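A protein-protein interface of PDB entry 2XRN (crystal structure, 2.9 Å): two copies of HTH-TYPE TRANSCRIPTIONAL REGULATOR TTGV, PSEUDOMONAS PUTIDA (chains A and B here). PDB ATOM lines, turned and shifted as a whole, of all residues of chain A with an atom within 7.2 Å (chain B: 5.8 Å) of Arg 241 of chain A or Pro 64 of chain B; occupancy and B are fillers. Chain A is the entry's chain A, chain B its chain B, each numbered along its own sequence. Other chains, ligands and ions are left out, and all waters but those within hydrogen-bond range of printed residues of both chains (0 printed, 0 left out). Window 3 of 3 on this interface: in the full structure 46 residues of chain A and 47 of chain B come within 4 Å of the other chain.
O of Leu 203 of chain A lies within hydrogen-bond range of N of Gly 67 of chain B (3.2 Å).
N of Tyr 205 of chain A lies close to NE2 of Gln 68 of chain B (3.5 Å).
The side-chain carboxylate (OE2) of Glu 52 of chain B lies within salt-bridge range of the guanidinium group (NE) of Arg 241 of chain A, 3.97 Å away.
The backbone carbonyl oxygen (O) of Tyr 202 of chain A sits close to the backbone carbonyl oxygen (O) of Gly 63 of chain B, 3.2 Å away.
The backbone carbonyl oxygen of Tyr 202 of chain A sits close to the backbone nitrogen of Pro 64 of chain B.
The backbone carbonyl oxygen (O) of Leu 203 of chain A lies close to the backbone carbonyl oxygen (O) of Pro 64 of chain B.
OD2 of Asp 200 of chain A is in salt-bridge range of NE of Arg 241 of chain A (3.4 Å).
N of Leu 203 of chain A lies close to OG1 of Thr 201 of chain A (3.4 Å).
O of Ile 239 of chain A lies close to N of Tyr 202 of chain A.
The backbone NH (N) of Gly 63 of chain B sits at hydrogen-bond distance from the backbone carbonyl oxygen (O) of Leu 50 of chain B.
The guanidinium group (NH1) of Arg 61 of chain B lies within salt-bridge range of the side-chain carboxylate (OE1) of Glu 52 of chain B (3.2 Å).
O of Pro 64 of chain B lies within hydrogen-bond range of NE2 of Gln 68 of chain B, 3.4 Å away.
Among the printed residues, merely in contact across the chains: Gly 204 of chain A with Gln 68 of chain B, Tyr 202 of chain A with Arg 61 of chain B, Arg 241 of chain A with Pro 64 of chain B, Tyr 202 of chain A with Glu 52 of chain B, Tyr 202 of chain A with Leu 62 of chain B, Ile 70 of chain A with Leu 66 of chain B, Gly 204 of chain A with Pro 64 of chain B, Leu 203 of chain A with Gly 63 of chain B and Gly 240 of chain A with Arg 61 of chain B.
Printed residues of chain B within 4 Å of Tyr 202 of chain A: Glu 52 (3.5 Å), Arg 61 (3.2 Å), Leu 62 (3.7 Å), Gly 63 (2.8 Å) and Pro 64 (2.8 Å).
Of the printed residues of chain B, Leu 203 of chain A touches Gly 63 (3.8 Å), Pro 64 (3.2 Å) and Gly 67 (3.2 Å).
Of the printed residues of chain B, Gly 240 of chain A touches Arg 61 (3.98 Å).
Of chain B, only Glu 52 and Pro 64 come within 4 Å of Arg 241 of chain A.
Of the printed residues of chain A, Gly 63 of chain B touches Tyr 202 and Leu 203.
Printed residues of chain A within 4 Å of Pro 64 of chain B: Tyr 202, Leu 203, Gly 204 and Arg 241.
The nearest printed residue of chain B that does not touch Arg 241 of chain A is Arg 61 of chain B (4.9 Å).
The nearest residue of chain A that does not touch Pro 64 of chain B is Thr 201 of chain A (4.6 Å).
Of the 11 printed residues of chain A, 7 touch a printed residue of chain B.
Printed residues of chain A that touch a printed residue of chain B: Ile 70, Tyr 202, Leu 203, Gly 204, Tyr 205, Gly 240 and Arg 241.
Hydrophobic or aromatic side chains of chain A within 4 Å of the printed part of chain B: Ile 70, Tyr 202 and Leu 203.
Hydrophobic or aromatic side chains of chain B within 4 Å of the printed part of chain A: Pro 64 and Leu 66.
Along chain B the printed residues that touch a printed residue of chain A span positions 52 to 68.
Among the printed residues, 15 pairs touch across the chains.
Among the printed residues, Asp or Glu carboxylates within 4 Å of a Lys or Arg side-chain nitrogen of the other chain: Arg 241 of chain A with Glu 52 of chain B.
No position is printed for both chains.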
ATOM      1  N   ILE A  70       8.728   4.853  35.610  1.00  0.00           N
ATOM      2  CA  ILE A  70       8.414   6.000  34.776  1.00  0.00           C
ATOM      3  C   ILE A  70       7.637   7.102  35.502  1.00  0.00           C
ATOM      4  O   ILE A  70       7.982   8.286  35.405  1.00  0.00           O
ATOM      5  CB  ILE A  70       7.605   5.552  33.555  1.00  0.00           C
ATOM      6  CG1 ILE A  70       8.533   5.265  32.384  1.00  0.00           C
ATOM      7  CG2 ILE A  70       6.631   6.618  33.154  1.00  0.00           C
ATOM      8  CD1 ILE A  70       9.274   6.496  31.912  1.00  0.00           C
ATOM      9  N   ASP A 200      12.007  16.963  21.900  1.00  0.00           N
ATOM     10  CA  ASP A 200      12.914  15.864  22.178  1.00  0.00           C
ATOM     11  C   ASP A 200      13.346  15.900  23.635  1.00  0.00           C
ATOM     12  O   ASP A 200      14.361  16.503  23.972  1.00  0.00           O
ATOM     13  CB  ASP A 200      14.147  15.951  21.280  1.00  0.00           C
ATOM     14  CG  ASP A 200      14.869  14.628  21.155  1.00  0.00           C
ATOM     15  OD1 ASP A 200      15.750  14.526  20.276  1.00  0.00           O
ATOM     16  OD2 ASP A 200      14.540  13.687  21.920  1.00  0.00           O
ATOM     17  N   THR A 201      12.573  15.257  24.500  1.00  0.00           N
ATOM     18  CA  THR A 201      12.894  15.260  25.916  1.00  0.00           C
ATOM     19  C   THR A 201      13.756  14.063  26.280  1.00  0.00           C
ATOM     20  O   THR A 201      13.869  13.100  25.522  1.00  0.00           O
ATOM     21  CB  THR A 201      11.634  15.233  26.786  1.00  0.00           C
ATOM     22  OG1 THR A 201      10.953  13.990  26.591  1.00  0.00           O
ATOM     23  CG2 THR A 201      10.709  16.383  26.420  1.00  0.00           C
ATOM     24  N   TYR A 202      14.359  14.125  27.458  1.00  0.00           N
ATOM     25  CA  TYR A 202      15.212  13.045  27.907  1.00  0.00           C
ATOM     26  C   TYR A 202      14.395  11.799  28.167  1.00  0.00           C
ATOM     27  O   TYR A 202      14.944  10.718  28.349  1.00  0.00           O
ATOM     28  CB  TYR A 202      15.954  13.449  29.173  1.00  0.00           C
ATOM     29  CG  TYR A 202      15.070  13.680  30.372  1.00  0.00           C
ATOM     30  CD1 TYR A 202      14.630  12.621  31.149  1.00  0.00           C
ATOM     31  CD2 TYR A 202      14.693  14.962  30.742  1.00  0.00           C
ATOM     32  CE1 TYR A 202      13.828  12.833  32.260  1.00  0.00           C
ATOM     33  CE2 TYR A 202      13.894  15.185  31.850  1.00  0.00           C
ATOM     34  CZ  TYR A 202      13.464  14.117  32.604  1.00  0.00           C
ATOM     35  OH  TYR A 202      12.669  14.343  33.705  1.00  0.00           O
ATOM     36  N   LEU A 203      13.078  11.948  28.186  1.00  0.00           N
ATOM     37  CA  LEU A 203      12.201  10.835  28.514  1.00  0.00           C
ATOM     38  C   LEU A 203      11.523  10.274  27.268  1.00  0.00           C
ATOM     39  O   LEU A 203      10.811   9.273  27.337  1.00  0.00           O
ATOM     40  CB  LEU A 203      11.161  11.277  29.543  1.00  0.00           C
ATOM     41  CG  LEU A 203      10.491  10.212  30.409  1.00  0.00           C
ATOM     42  CD1 LEU A 203      11.515   9.303  31.085  1.00  0.00           C
ATOM     43  CD2 LEU A 203       9.613  10.895  31.447  1.00  0.00           C
ATOM     44  N   GLY A 204      11.754  10.920  26.128  1.00  0.00           N
ATOM     45  CA  GLY A 204      11.156  10.490  24.874  1.00  0.00           C
ATOM     46  C   GLY A 204      10.656  11.633  24.007  1.00  0.00           C
ATOM     47  O   GLY A 204      10.965  12.795  24.268  1.00  0.00           O
ATOM     48  N   TYR A 205       9.884  11.305  22.972  1.00  0.00           N
ATOM     49  CA  TYR A 205       9.377  12.324  22.050  1.00  0.00           C
ATOM     50  C   TYR A 205       7.946  12.777  22.367  1.00  0.00           C
ATOM     51  O   TYR A 205       7.048  11.957  22.582  1.00  0.00           O
ATOM     52  CB  TYR A 205       9.444  11.835  20.600  1.00  0.00           C
ATOM     53  CG  TYR A 205      10.835  11.570  20.078  1.00  0.00           C
ATOM     54  CD1 TYR A 205      11.731  12.608  19.872  1.00  0.00           C
ATOM     55  CD2 TYR A 205      11.245  10.281  19.764  1.00  0.00           C
ATOM     56  CE1 TYR A 205      13.003  12.368  19.385  1.00  0.00           C
ATOM     57  CE2 TYR A 205      12.514  10.032  19.275  1.00  0.00           C
ATOM     58  CZ  TYR A 205      13.389  11.078  19.089  1.00  0.00           C
ATOM     59  OH  TYR A 205      14.653  10.834  18.606  1.00  0.00           O
ATOM     60  N   GLU A 236      12.987  22.525  25.415  1.00  0.00           N
ATOM     61  CA  GLU A 236      14.149  21.647  25.271  1.00  0.00           C
ATOM     62  C   GLU A 236      15.363  22.155  26.030  1.00  0.00           C
ATOM     63  O   GLU A 236      16.144  21.368  26.565  1.00  0.00           O
ATOM     64  CB  GLU A 236      14.514  21.448  23.802  1.00  0.00           C
ATOM     65  CG  GLU A 236      13.691  20.389  23.116  1.00  0.00           C
ATOM     66  CD  GLU A 236      14.026  20.263  21.659  1.00  0.00           C
ATOM     67  OE1 GLU A 236      14.963  20.950  21.212  1.00  0.00           O
ATOM     68  OE2 GLU A 236      13.354  19.478  20.962  1.00  0.00           O
ATOM     69  N   ILE A 239      14.559  20.868  29.331  1.00  0.00           N
ATOM     70  CA  ILE A 239      14.113  19.485  29.507  1.00  0.00           C
ATOM     71  C   ILE A 239      14.611  18.519  28.429  1.00  0.00           C
ATOM     72  O   ILE A 239      14.248  17.344  28.425  1.00  0.00           O
ATOM     73  CB  ILE A 239      12.565  19.544  29.453  1.00  0.00           C
ATOM     74  CG1 ILE A 239      11.930  18.319  30.089  1.00  0.00           C
ATOM     75  CG2 ILE A 239      12.069  19.644  28.023  1.00  0.00           C
ATOM     76  CD1 ILE A 239      10.545  18.057  29.529  1.00  0.00           C
ATOM     77  N   GLY A 240      15.442  19.015  27.517  1.00  0.00           N
ATOM     78  CA  GLY A 240      15.938  18.214  26.409  1.00  0.00           C
ATOM     79  C   GLY A 240      16.956  17.166  26.811  1.00  0.00           C
ATOM     80  O   GLY A 240      17.194  16.941  27.999  1.00  0.00           O
ATOM     81  N   ARG A 241      17.573  16.535  25.818  1.00  0.00           N
ATOM     82  CA  ARG A 241      18.504  15.434  26.062  1.00  0.00           C
ATOM     83  C   ARG A 241      19.933  15.720  25.584  1.00  0.00           C
ATOM     84  O   ARG A 241      20.843  14.899  25.766  1.00  0.00           O
ATOM     85  CB  ARG A 241      17.984  14.164  25.393  1.00  0.00           C
ATOM     86  CG  ARG A 241      17.617  14.367  23.950  1.00  0.00           C
ATOM     87  CD  ARG A 241      18.166  13.267  23.080  1.00  0.00           C
ATOM     88  NE  ARG A 241      17.302  12.098  23.054  1.00  0.00           N
ATOM     89  CZ  ARG A 241      17.099  11.357  21.969  1.00  0.00           C
ATOM     90  NH1 ARG A 241      17.701  11.682  20.832  1.00  0.00           N
ATOM     91  NH2 ARG A 241      16.296  10.299  22.015  1.00  0.00           N
ATOM     92  N   PHE B  49      19.891   3.830  25.598  1.00  0.00           N
ATOM     93  CA  PHE B  49      19.087   5.021  25.862  1.00  0.00           C
ATOM     94  C   PHE B  49      18.088   4.819  26.990  1.00  0.00           C
ATOM     95  O   PHE B  49      17.145   5.595  27.135  1.00  0.00           O
ATOM     96  CB  PHE B  49      18.361   5.481  24.602  1.00  0.00           C
ATOM     97  CG  PHE B  49      19.275   5.791  23.464  1.00  0.00           C
ATOM     98  CD1 PHE B  49      19.808   7.061  23.313  1.00  0.00           C
ATOM     99  CD2 PHE B  49      19.611   4.811  22.544  1.00  0.00           C
ATOM    100  CE1 PHE B  49      20.654   7.346  22.264  1.00  0.00           C
ATOM    101  CE2 PHE B  49      20.453   5.090  21.492  1.00  0.00           C
ATOM    102  CZ  PHE B  49      20.975   6.361  21.352  1.00  0.00           C
ATOM    103  N   LEU B  50      18.291   3.775  27.782  1.00  0.00           N
ATOM    104  CA  LEU B  50      17.481   3.578  28.970  1.00  0.00           C
ATOM    105  C   LEU B  50      17.980   4.498  30.073  1.00  0.00           C
ATOM    106  O   LEU B  50      17.318   4.667  31.092  1.00  0.00           O
ATOM    107  CB  LEU B  50      17.521   2.119  29.416  1.00  0.00           C
ATOM    108  CG  LEU B  50      17.086   1.157  28.311  1.00  0.00           C
ATOM    109  CD1 LEU B  50      17.470  -0.277  28.635  1.00  0.00           C
ATOM    110  CD2 LEU B  50      15.592   1.284  28.056  1.00  0.00           C
ATOM    111  N   VAL B  51      19.152   5.092  29.858  1.00  0.00           N
ATOM    112  CA  VAL B  51      19.722   6.051  30.800  1.00  0.00           C
ATOM    113  C   VAL B  51      20.502   7.142  30.061  1.00  0.00           C
ATOM    114  O   VAL B  51      20.966   6.939  28.938  1.00  0.00           O
ATOM    115  CB  VAL B  51      20.654   5.373  31.840  1.00  0.00           C
ATOM    116  CG1 VAL B  51      21.255   6.409  32.766  1.00  0.00           C
ATOM    117  CG2 VAL B  51      19.903   4.332  32.659  1.00  0.00           C
ATOM    118  N   GLU B  52      20.624   8.303  30.696  1.00  0.00           N
ATOM    119  CA  GLU B  52      21.408   9.415  30.182  1.00  0.00           C
ATOM    120  C   GLU B  52      22.289   9.975  31.287  1.00  0.00           C
ATOM    121  O   GLU B  52      21.981   9.826  32.473  1.00  0.00           O
ATOM    122  CB  GLU B  52      20.496  10.528  29.681  1.00  0.00           C
ATOM    123  CG  GLU B  52      20.081  10.398  28.241  1.00  0.00           C
ATOM    124  CD  GLU B  52      19.493  11.688  27.707  1.00  0.00           C
ATOM    125  OE1 GLU B  52      19.250  12.610  28.522  1.00  0.00           O
ATOM    126  OE2 GLU B  52      19.288  11.780  26.478  1.00  0.00           O
ATOM    127  N   ARG B  61      20.372   9.858  34.912  1.00  0.00           N
ATOM    128  CA  ARG B  61      18.923   9.886  35.067  1.00  0.00           C
ATOM    129  C   ARG B  61      18.313   9.054  33.942  1.00  0.00           C
ATOM    130  O   ARG B  61      19.031   8.636  33.044  1.00  0.00           O
ATOM    131  CB  ARG B  61      18.408  11.331  35.074  1.00  0.00           C
ATOM    132  CG  ARG B  61      17.436  11.660  33.967  1.00  0.00           C
ATOM    133  CD  ARG B  61      18.068  12.534  32.895  1.00  0.00           C
ATOM    134  NE  ARG B  61      17.686  13.935  33.037  1.00  0.00           N
ATOM    135  CZ  ARG B  61      17.838  14.848  32.083  1.00  0.00           C
ATOM    136  NH1 ARG B  61      18.361  14.504  30.916  1.00  0.00           N
ATOM    137  NH2 ARG B  61      17.465  16.102  32.295  1.00  0.00           N
ATOM    138  N   LEU B  62      17.012   8.783  33.994  1.00  0.00           N
ATOM    139  CA  LEU B  62      16.398   7.914  32.987  1.00  0.00           C
ATOM    140  C   LEU B  62      16.514   8.505  31.579  1.00  0.00           C
ATOM    141  O   LEU B  62      16.839   9.684  31.419  1.00  0.00           O
ATOM    142  CB  LEU B  62      14.944   7.604  33.341  1.00  0.00           C
ATOM    143  CG  LEU B  62      14.741   6.957  34.713  1.00  0.00           C
ATOM    144  CD1 LEU B  62      13.273   6.806  35.050  1.00  0.00           C
ATOM    145  CD2 LEU B  62      15.436   5.610  34.767  1.00  0.00           C
ATOM    146  N   GLY B  63      16.252   7.688  30.563  1.00  0.00           N
ATOM    147  CA  GLY B  63      16.489   8.096  29.189  1.00  0.00           C
ATOM    148  C   GLY B  63      15.292   7.975  28.267  1.00  0.00           C
ATOM    149  O   GLY B  63      14.206   7.603  28.702  1.00  0.00           O
ATOM    150  N   PRO B  64      15.493   8.281  26.978  1.00  0.00           N
ATOM    151  CA  PRO B  64      14.452   8.309  25.944  1.00  0.00           C
ATOM    152  C   PRO B  64      13.683   7.000  25.765  1.00  0.00           C
ATOM    153  O   PRO B  64      12.460   6.994  25.904  1.00  0.00           O
ATOM    154  CB  PRO B  64      15.241   8.624  24.671  1.00  0.00           C
ATOM    155  CG  PRO B  64      16.448   9.337  25.146  1.00  0.00           C
ATOM    156  CD  PRO B  64      16.803   8.684  26.444  1.00  0.00           C
ATOM    157  N   ALA B  65      14.387   5.916  25.450  1.00  0.00           N
ATOM    158  CA  ALA B  65      13.745   4.635  25.158  1.00  0.00           C
ATOM    159  C   ALA B  65      12.549   4.368  26.067  1.00  0.00           C
ATOM    160  O   ALA B  65      11.501   3.891  25.615  1.00  0.00           O
ATOM    161  CB  ALA B  65      14.745   3.511  25.259  1.00  0.00           C
ATOM    162  N   LEU B  66      12.711   4.685  27.346  1.00  0.00           N
ATOM    163  CA  LEU B  66      11.644   4.493  28.320  1.00  0.00           C
ATOM    164  C   LEU B  66      10.267   4.853  27.775  1.00  0.00           C
ATOM    165  O   LEU B  66       9.378   4.004  27.710  1.00  0.00           O
ATOM    166  CB  LEU B  66      11.924   5.301  29.582  1.00  0.00           C
ATOM    167  CG  LEU B  66      12.381   4.436  30.747  1.00  0.00           C
ATOM    168  CD1 LEU B  66      13.237   3.302  30.226  1.00  0.00           C
ATOM    169  CD2 LEU B  66      13.138   5.274  31.761  1.00  0.00           C
ATOM    170  N   GLY B  67      10.096   6.113  27.389  1.00  0.00           N
ATOM    171  CA  GLY B  67       8.836   6.568  26.835  1.00  0.00           C
ATOM    172  C   GLY B  67       8.242   5.556  25.879  1.00  0.00           C
ATOM    173  O   GLY B  67       7.142   5.041  26.096  1.00  0.00           O
ATOM    174  N   GLN B  68       8.996   5.230  24.838  1.00  0.00           N
ATOM    175  CA  GLN B  68       8.478   4.407  23.755  1.00  0.00           C
ATOM    176  C   GLN B  68       8.099   2.992  24.194  1.00  0.00           C
ATOM    177  O   GLN B  68       7.295   2.328  23.535  1.00  0.00           O
ATOM    178  CB  GLN B  68       9.479   4.385  22.603  1.00  0.00           C
ATOM    179  CG  GLN B  68      10.461   5.564  22.636  1.00  0.00           C
ATOM    180  CD  GLN B  68       9.788   6.925  22.858  1.00  0.00           C
ATOM    181  OE1 GLN B  68       8.581   7.082  22.666  1.00  0.00           O
ATOM    182  NE2 GLN B  68      10.579   7.911  23.267  1.00  0.00           N
